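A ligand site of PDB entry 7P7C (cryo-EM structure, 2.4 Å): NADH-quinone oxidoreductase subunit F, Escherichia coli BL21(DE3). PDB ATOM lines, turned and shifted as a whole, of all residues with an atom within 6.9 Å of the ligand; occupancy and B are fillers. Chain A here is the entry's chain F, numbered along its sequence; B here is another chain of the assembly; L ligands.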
ATOM      1  N   ILE A 176      11.177  11.911   5.347  1.00  0.00           N
ATOM      2  CA  ILE A 176      10.622  11.387   4.094  1.00  0.00           C
ATOM      3  C   ILE A 176      11.602  11.533   2.935  1.00  0.00           C
ATOM      4  O   ILE A 176      11.497  10.807   1.947  1.00  0.00           O
ATOM      5  CB  ILE A 176       9.272  12.070   3.801  1.00  0.00           C
ATOM      6  CG1 ILE A 176       8.469  11.305   2.740  1.00  0.00           C
ATOM      7  CG2 ILE A 176       9.476  13.517   3.373  1.00  0.00           C
ATOM      8  CD1 ILE A 176       8.471   9.795   2.907  1.00  0.00           C
ATOM      9  N   GLU A 179      13.258   8.336   1.385  1.00  0.00           N
ATOM     10  CA  GLU A 179      12.596   7.580   0.337  1.00  0.00           C
ATOM     11  C   GLU A 179      13.100   8.024  -1.030  1.00  0.00           C
ATOM     12  O   GLU A 179      13.261   9.220  -1.272  1.00  0.00           O
ATOM     13  CB  GLU A 179      11.079   7.756   0.437  1.00  0.00           C
ATOM     14  CG  GLU A 179      10.267   6.662  -0.227  1.00  0.00           C
ATOM     15  CD  GLU A 179       9.958   6.950  -1.674  1.00  0.00           C
ATOM     16  OE1 GLU A 179      10.144   8.110  -2.096  1.00  0.00           O
ATOM     17  OE2 GLU A 179       9.541   6.021  -2.397  1.00  0.00           O
ATOM     18  N   ALA A 192       9.572  17.287  -0.712  1.00  0.00           N
ATOM     19  CA  ALA A 192       9.978  15.883  -0.821  1.00  0.00           C
ATOM     20  C   ALA A 192       8.776  14.943  -0.741  1.00  0.00           C
ATOM     21  O   ALA A 192       8.706  14.047   0.102  1.00  0.00           O
ATOM     22  CB  ALA A 192      11.009  15.568   0.248  1.00  0.00           C
ATOM     23  N   ASN A 193       7.823  15.157  -1.634  1.00  0.00           N
ATOM     24  CA  ASN A 193       6.809  14.144  -1.836  1.00  0.00           C
ATOM     25  C   ASN A 193       7.384  13.020  -2.693  1.00  0.00           C
ATOM     26  O   ASN A 193       8.145  13.277  -3.625  1.00  0.00           O
ATOM     27  CB  ASN A 193       5.580  14.736  -2.520  1.00  0.00           C
ATOM     28  CG  ASN A 193       4.975  15.897  -1.771  1.00  0.00           C
ATOM     29  OD1 ASN A 193       5.011  17.027  -2.231  1.00  0.00           O
ATOM     30  ND2 ASN A 193       4.418  15.612  -0.599  1.00  0.00           N
ATOM     31  N   PRO A 194       7.054  11.763  -2.385  1.00  0.00           N
ATOM     32  CA  PRO A 194       7.469  10.669  -3.255  1.00  0.00           C
ATOM     33  C   PRO A 194       6.704  10.677  -4.570  1.00  0.00           C
ATOM     34  O   PRO A 194       5.729  11.414  -4.762  1.00  0.00           O
ATOM     35  CB  PRO A 194       7.154   9.420  -2.434  1.00  0.00           C
ATOM     36  CG  PRO A 194       6.189   9.853  -1.430  1.00  0.00           C
ATOM     37  CD  PRO A 194       6.443  11.288  -1.141  1.00  0.00           C
ATOM     38  N   PHE A 343       6.285   9.192  13.488  1.00  0.00           N
ATOM     39  CA  PHE A 343       5.808   8.841  12.157  1.00  0.00           C
ATOM     40  C   PHE A 343       4.721   9.814  11.673  1.00  0.00           C
ATOM     41  O   PHE A 343       4.701  10.172  10.496  1.00  0.00           O
ATOM     42  CB  PHE A 343       5.280   7.411  12.146  1.00  0.00           C
ATOM     43  CG  PHE A 343       6.356   6.374  12.085  1.00  0.00           C
ATOM     44  CD1 PHE A 343       7.284   6.378  11.052  1.00  0.00           C
ATOM     45  CD2 PHE A 343       6.457   5.387  13.053  1.00  0.00           C
ATOM     46  CE1 PHE A 343       8.279   5.432  10.985  1.00  0.00           C
ATOM     47  CE2 PHE A 343       7.459   4.436  12.992  1.00  0.00           C
ATOM     48  CZ  PHE A 343       8.369   4.462  11.962  1.00  0.00           C
ATOM     49  N   GLU A 346       6.341  13.069  10.670  1.00  0.00           N
ATOM     50  CA  GLU A 346       7.208  12.953   9.510  1.00  0.00           C
ATOM     51  C   GLU A 346       6.450  12.561   8.253  1.00  0.00           C
ATOM     52  O   GLU A 346       7.072  12.268   7.228  1.00  0.00           O
ATOM     53  CB  GLU A 346       8.330  11.959   9.776  1.00  0.00           C
ATOM     54  CG  GLU A 346       9.361  12.463  10.760  1.00  0.00           C
ATOM     55  CD  GLU A 346       9.877  13.844  10.415  1.00  0.00           C
ATOM     56  OE1 GLU A 346      10.364  14.041   9.290  1.00  0.00           O
ATOM     57  OE2 GLU A 346       9.787  14.741  11.283  1.00  0.00           O
ATOM     58  N   SER A 347       5.119  12.546   8.311  1.00  0.00           N
ATOM     59  CA  SER A 347       4.311  12.394   7.113  1.00  0.00           C
ATOM     60  C   SER A 347       4.569  13.553   6.166  1.00  0.00           C
ATOM     61  O   SER A 347       4.707  14.695   6.590  1.00  0.00           O
ATOM     62  CB  SER A 347       2.836  12.327   7.493  1.00  0.00           C
ATOM     63  OG  SER A 347       2.005  12.313   6.344  1.00  0.00           O
ATOM     64  N   CYS A 348       4.649  13.254   4.875  1.00  0.00           N
ATOM     65  CA  CYS A 348       4.848  14.323   3.911  1.00  0.00           C
ATOM     66  C   CYS A 348       3.551  15.047   3.568  1.00  0.00           C
ATOM     67  O   CYS A 348       3.605  16.128   2.978  1.00  0.00           O
ATOM     68  CB  CYS A 348       5.511  13.791   2.647  1.00  0.00           C
ATOM     69  SG  CYS A 348       4.374  13.128   1.438  1.00  0.00           S
ATOM     70  N   GLY A 349       2.412  14.492   3.948  1.00  0.00           N
ATOM     71  CA  GLY A 349       1.132  15.146   3.740  1.00  0.00           C
ATOM     72  C   GLY A 349       0.492  14.912   2.399  1.00  0.00           C
ATOM     73  O   GLY A 349      -0.555  15.515   2.117  1.00  0.00           O
ATOM     74  N   TRP A 350       1.071  14.063   1.543  1.00  0.00           N
ATOM     75  CA  TRP A 350       0.526  13.857   0.215  1.00  0.00           C
ATOM     76  C   TRP A 350      -0.788  13.088   0.251  1.00  0.00           C
ATOM     77  O   TRP A 350      -1.767  13.488  -0.377  1.00  0.00           O
ATOM     78  CB  TRP A 350       1.542  13.129  -0.664  1.00  0.00           C
ATOM     79  CG  TRP A 350       1.083  12.809  -2.046  1.00  0.00           C
ATOM     80  CD1 TRP A 350       0.857  11.565  -2.565  1.00  0.00           C
ATOM     81  CD2 TRP A 350       0.808  13.735  -3.098  1.00  0.00           C
ATOM     82  NE1 TRP A 350       0.447  11.662  -3.868  1.00  0.00           N
ATOM     83  CE2 TRP A 350       0.416  12.984  -4.218  1.00  0.00           C
ATOM     84  CE3 TRP A 350       0.861  15.124  -3.199  1.00  0.00           C
ATOM     85  CZ2 TRP A 350       0.073  13.582  -5.431  1.00  0.00           C
ATOM     86  CZ3 TRP A 350       0.516  15.717  -4.395  1.00  0.00           C
ATOM     87  CH2 TRP A 350       0.130  14.952  -5.500  1.00  0.00           C
ATOM     88  N   CYS A 351      -0.831  11.977   0.979  1.00  0.00           N
ATOM     89  CA  CYS A 351      -1.945  11.056   0.847  1.00  0.00           C
ATOM     90  C   CYS A 351      -2.709  10.895   2.155  1.00  0.00           C
ATOM     91  O   CYS A 351      -2.140  10.947   3.245  1.00  0.00           O
ATOM     92  CB  CYS A 351      -1.476   9.705   0.285  1.00  0.00           C
ATOM     93  SG  CYS A 351      -0.679   8.559   1.379  1.00  0.00           S
ATOM     94  N   THR A 352      -4.016  10.694   2.003  1.00  0.00           N
ATOM     95  CA  THR A 352      -4.964  10.762   3.117  1.00  0.00           C
ATOM     96  C   THR A 352      -4.722   9.760   4.254  1.00  0.00           C
ATOM     97  O   THR A 352      -4.760  10.183   5.420  1.00  0.00           O
ATOM     98  CB  THR A 352      -6.392  10.622   2.581  1.00  0.00           C
ATOM     99  OG1 THR A 352      -6.637  11.635   1.596  1.00  0.00           O
ATOM    100  CG2 THR A 352      -7.411  10.752   3.690  1.00  0.00           C
ATOM    101  N   PRO A 353      -4.502   8.446   4.019  1.00  0.00           N
ATOM    102  CA  PRO A 353      -4.428   7.518   5.171  1.00  0.00           C
ATOM    103  C   PRO A 353      -3.300   7.819   6.140  1.00  0.00           C
ATOM    104  O   PRO A 353      -3.534   7.894   7.333  1.00  0.00           O
ATOM    105  CB  PRO A 353      -4.273   6.154   4.501  1.00  0.00           C
ATOM    106  CG  PRO A 353      -4.823   6.326   3.164  1.00  0.00           C
ATOM    107  CD  PRO A 353      -4.360   7.673   2.768  1.00  0.00           C
ATOM    108  N   CYS A 354      -2.092   8.068   5.627  1.00  0.00           N
ATOM    109  CA  CYS A 354      -0.986   8.438   6.503  1.00  0.00           C
ATOM    110  C   CYS A 354      -1.250   9.767   7.204  1.00  0.00           C
ATOM    111  O   CYS A 354      -1.314   9.815   8.436  1.00  0.00           O
ATOM    112  CB  CYS A 354       0.296   8.476   5.666  1.00  0.00           C
ATOM    113  SG  CYS A 354       1.834   9.136   6.326  1.00  0.00           S
ATOM    114  N   ARG A 355      -1.570  10.801   6.413  1.00  0.00           N
ATOM    115  CA  ARG A 355      -1.677  12.167   6.903  1.00  0.00           C
ATOM    116  C   ARG A 355      -2.790  12.332   7.943  1.00  0.00           C
ATOM    117  O   ARG A 355      -2.618  13.057   8.921  1.00  0.00           O
ATOM    118  CB  ARG A 355      -1.908  13.129   5.721  1.00  0.00           C
ATOM    119  CG  ARG A 355      -2.531  14.460   6.085  1.00  0.00           C
ATOM    120  CD  ARG A 355      -2.840  15.329   4.871  1.00  0.00           C
ATOM    121  NE  ARG A 355      -4.174  15.068   4.371  1.00  0.00           N
ATOM    122  CZ  ARG A 355      -4.450  14.488   3.211  1.00  0.00           C
ATOM    123  NH1 ARG A 355      -3.486  14.156   2.376  1.00  0.00           N
ATOM    124  NH2 ARG A 355      -5.712  14.248   2.887  1.00  0.00           N
ATOM    125  N   LEU A 358      -2.494   8.554  10.925  1.00  0.00           N
ATOM    126  CA  LEU A 358      -1.453   8.533  11.954  1.00  0.00           C
ATOM    127  C   LEU A 358      -1.725   9.478  13.129  1.00  0.00           C
ATOM    128  O   LEU A 358      -1.505   9.047  14.272  1.00  0.00           O
ATOM    129  CB  LEU A 358      -0.082   8.794  11.309  1.00  0.00           C
ATOM    130  CG  LEU A 358       0.446   7.641  10.450  1.00  0.00           C
ATOM    131  CD1 LEU A 358       1.812   7.958   9.890  1.00  0.00           C
ATOM    132  CD2 LEU A 358       0.487   6.357  11.271  1.00  0.00           C
ATOM    133  N   THR A 393      -1.573   3.331   0.832  1.00  0.00           N
ATOM    134  CA  THR A 393      -0.958   4.654   0.863  1.00  0.00           C
ATOM    135  C   THR A 393      -0.064   4.832  -0.360  1.00  0.00           C
ATOM    136  O   THR A 393       0.259   3.887  -1.073  1.00  0.00           O
ATOM    137  CB  THR A 393      -0.162   4.856   2.149  1.00  0.00           C
ATOM    138  OG1 THR A 393       0.888   3.878   2.219  1.00  0.00           O
ATOM    139  CG2 THR A 393      -1.068   4.698   3.351  1.00  0.00           C
ATOM    140  N   PHE A 394       0.345   6.084  -0.576  1.00  0.00           N
ATOM    141  CA  PHE A 394       1.096   6.418  -1.783  1.00  0.00           C
ATOM    142  C   PHE A 394       2.536   5.928  -1.706  1.00  0.00           C
ATOM    143  O   PHE A 394       3.131   5.626  -2.743  1.00  0.00           O
ATOM    144  CB  PHE A 394       1.041   7.922  -2.013  1.00  0.00           C
ATOM    145  CG  PHE A 394       1.589   8.359  -3.335  1.00  0.00           C
ATOM    146  CD1 PHE A 394       0.813   8.245  -4.490  1.00  0.00           C
ATOM    147  CD2 PHE A 394       2.853   8.899  -3.439  1.00  0.00           C
ATOM    148  CE1 PHE A 394       1.312   8.654  -5.704  1.00  0.00           C
ATOM    149  CE2 PHE A 394       3.359   9.304  -4.648  1.00  0.00           C
ATOM    150  CZ  PHE A 394       2.581   9.186  -5.786  1.00  0.00           C
ATOM    151  N   CYS A 395       3.111   5.842  -0.506  1.00  0.00           N
ATOM    152  CA  CYS A 395       4.461   5.341  -0.347  1.00  0.00           C
ATOM    153  C   CYS A 395       4.515   4.456   0.897  1.00  0.00           C
ATOM    154  O   CYS A 395       3.520   4.285   1.600  1.00  0.00           O
ATOM    155  CB  CYS A 395       5.488   6.475  -0.276  1.00  0.00           C
ATOM    156  SG  CYS A 395       5.843   7.090   1.375  1.00  0.00           S
ATOM    157  N   ALA A 396       5.695   3.905   1.166  1.00  0.00           N
ATOM    158  CA  ALA A 396       5.880   2.878   2.177  1.00  0.00           C
ATOM    159  C   ALA A 396       6.131   3.431   3.571  1.00  0.00           C
ATOM    160  O   ALA A 396       6.476   2.663   4.474  1.00  0.00           O
ATOM    161  CB  ALA A 396       7.037   1.962   1.784  1.00  0.00           C
ATOM    162  N   HIS A 397       5.966   4.740   3.771  1.00  0.00           N
ATOM    163  CA  HIS A 397       6.203   5.340   5.080  1.00  0.00           C
ATOM    164  C   HIS A 397       5.147   4.902   6.098  1.00  0.00           C
ATOM    165  O   HIS A 397       5.477   4.575   7.245  1.00  0.00           O
ATOM    166  CB  HIS A 397       6.244   6.859   4.956  1.00  0.00           C
ATOM    167  CG  HIS A 397       6.123   7.576   6.261  1.00  0.00           C
ATOM    168  ND1 HIS A 397       4.930   8.082   6.722  1.00  0.00           N
ATOM    169  CD2 HIS A 397       7.048   7.878   7.193  1.00  0.00           C
ATOM    170  CE1 HIS A 397       5.133   8.668   7.886  1.00  0.00           C
ATOM    171  NE2 HIS A 397       6.408   8.557   8.197  1.00  0.00           N
ATOM    172  N   ALA A 398       3.879   4.886   5.697  1.00  0.00           N
ATOM    173  CA  ALA A 398       2.792   4.506   6.588  1.00  0.00           C
ATOM    174  C   ALA A 398       2.718   3.013   6.912  1.00  0.00           C
ATOM    175  O   ALA A 398       2.344   2.677   8.052  1.00  0.00           O
ATOM    176  CB  ALA A 398       1.454   5.002   6.028  1.00  0.00           C
ATOM    177  N   PRO A 399       3.002   2.068   5.984  1.00  0.00           N
ATOM    178  CA  PRO A 399       3.156   0.675   6.428  1.00  0.00           C
ATOM    179  C   PRO A 399       4.243   0.479   7.473  1.00  0.00           C
ATOM    180  O   PRO A 399       4.040  -0.251   8.448  1.00  0.00           O
ATOM    181  CB  PRO A 399       3.482  -0.063   5.125  1.00  0.00           C
ATOM    182  CG  PRO A 399       2.810   0.711   4.093  1.00  0.00           C
ATOM    183  CD  PRO A 399       2.911   2.134   4.504  1.00  0.00           C
ATOM    184  N   ALA B  43      -3.404  11.039  -4.915  1.00  0.00           N
ATOM    185  CA  ALA B  43      -3.195  11.636  -3.610  1.00  0.00           C
ATOM    186  C   ALA B  43      -4.264  11.207  -2.603  1.00  0.00           C
ATOM    187  O   ALA B  43      -3.953  10.620  -1.571  1.00  0.00           O
ATOM    188  CB  ALA B  43      -3.150  13.164  -3.714  1.00  0.00           C
ATOM    189  N   ARG B  45      -6.543   8.933  -2.309  1.00  0.00           N
ATOM    190  CA  ARG B  45      -6.781   7.499  -2.092  1.00  0.00           C
ATOM    191  C   ARG B  45      -8.263   7.160  -1.935  1.00  0.00           C
ATOM    192  O   ARG B  45      -8.611   6.116  -1.385  1.00  0.00           O
ATOM    193  CB  ARG B  45      -5.983   6.962  -0.885  1.00  0.00           C
ATOM    194  CG  ARG B  45      -4.557   7.454  -0.784  1.00  0.00           C
ATOM    195  CD  ARG B  45      -3.746   7.200  -2.039  1.00  0.00           C
ATOM    196  NE  ARG B  45      -3.336   5.808  -2.145  1.00  0.00           N
ATOM    197  CZ  ARG B  45      -2.515   5.352  -3.083  1.00  0.00           C
ATOM    198  NH1 ARG B  45      -2.011   6.157  -4.008  1.00  0.00           N
ATOM    199  NH2 ARG B  45      -2.208   4.065  -3.104  1.00  0.00           N
ATOM    200  N   HIS B 175       2.943  17.610   7.452  1.00  0.00           N
ATOM    201  CA  HIS B 175       2.137  16.399   7.545  1.00  0.00           C
ATOM    202  C   HIS B 175       0.623  16.558   7.539  1.00  0.00           C
ATOM    203  O   HIS B 175      -0.004  16.287   6.520  1.00  0.00           O
ATOM    204  CB  HIS B 175       2.548  15.757   8.870  1.00  0.00           C
ATOM    205  CG  HIS B 175       2.944  16.778   9.901  1.00  0.00           C
ATOM    206  ND1 HIS B 175       2.029  17.393  10.729  1.00  0.00           N
ATOM    207  CD2 HIS B 175       4.145  17.325  10.209  1.00  0.00           C
ATOM    208  CE1 HIS B 175       2.654  18.261  11.505  1.00  0.00           C
ATOM    209  NE2 HIS B 175       3.940  18.238  11.211  1.00  0.00           N
HETATM  210 FE1  LIG L   1       1.488   9.214   1.930  1.00  0.00          FE
HETATM  211 FE2  LIG L   1       2.725   9.472   4.202  1.00  0.00          FE
HETATM  212 FE3  LIG L   1       4.150   8.516   2.078  1.00  0.00          FE
HETATM  213 FE4  LIG L   1       3.527  11.079   2.140  1.00  0.00          FE
HETATM  214  S1  LIG L   1       4.898  10.014   3.660  1.00  0.00           S
HETATM  215  S2  LIG L   1       3.115   9.667   0.364  1.00  0.00           S
HETATM  216  S3  LIG L   1       1.488  11.130   3.198  1.00  0.00           S
HETATM  217  S4  LIG L   1       2.396   7.471   3.117  1.00  0.00           S
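SG of Cys 348 sits close to ND2 of Asn 193, at 3.2 Å.
O of Gly 349 is in hydrogen-bond range of NH1 of Arg 355 (3.2 Å).
A ring nitrogen (NE2) of His 397 lies close to the backbone carbonyl oxygen of Phe 343, at 3.3 Å.
The backbone NH (N) of Gly 349 sits close to the side-chain hydroxyl (OG) of Ser 347, at 3.3 Å.
SG of Cys 348 lies close to N of Trp 350.
The side-chain sulfur of Cys 354 lies close to the side-chain hydroxyl of Ser 347 (3.2 Å).
O of Trp 350 is in hydrogen-bond range of NH1 of Arg 355 (3.3 Å).
The side-chain sulfur (SG) of Cys 354 sits close to a ring nitrogen (ND1) of His 397, 3.3 Å away.
Ile 176 touches the ligand.
CG of Pro 194 touches S2 of the ligand, at 3.6 Å.
CB of Thr 393 touches S4 of the ligand (3.8 Å).
CB of Phe 394 touches S2 of the ligand, at 3.6 Å.
Ala 398 touches the ligand (CB to S4, 3.9 Å).
Hydrophobic or aromatic side chains that line the ligand: Ile 176, Pro 194, Trp 350, Phe 394, His 397 and Ala 398.
ND1 of His 397 sits close to S1 of the ligand, 3.6 Å away.
The backbone NH (N) of Cys 348 lies close to a sulfur (S1) of the ligand (3.5 Å).
N of Gly 349 sits close to S3 of the ligand (3.6 Å).
N of Cys 351 sits close to S3 of the ligand (3.3 Å).
The side-chain hydroxyl (OG) of Ser 347 sits close to a sulfur (S3) of the ligand (3.4 Å).
The side-chain sulfur (SG) of Cys 351 binds an iron atom (FE1) of the ligand (2.3 Å).
An iron atom (FE3) of the ligand is bound by the side-chain sulfur of Cys 395 (2.3 Å).
The side-chain sulfur (SG) of Cys 348 binds an iron atom (FE4) of the ligand.
SG of Cys 354 binds FE2 of the ligand (2.3 Å).
S3 of the ligand sits close to N of Trp 350, at 3.4 Å.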
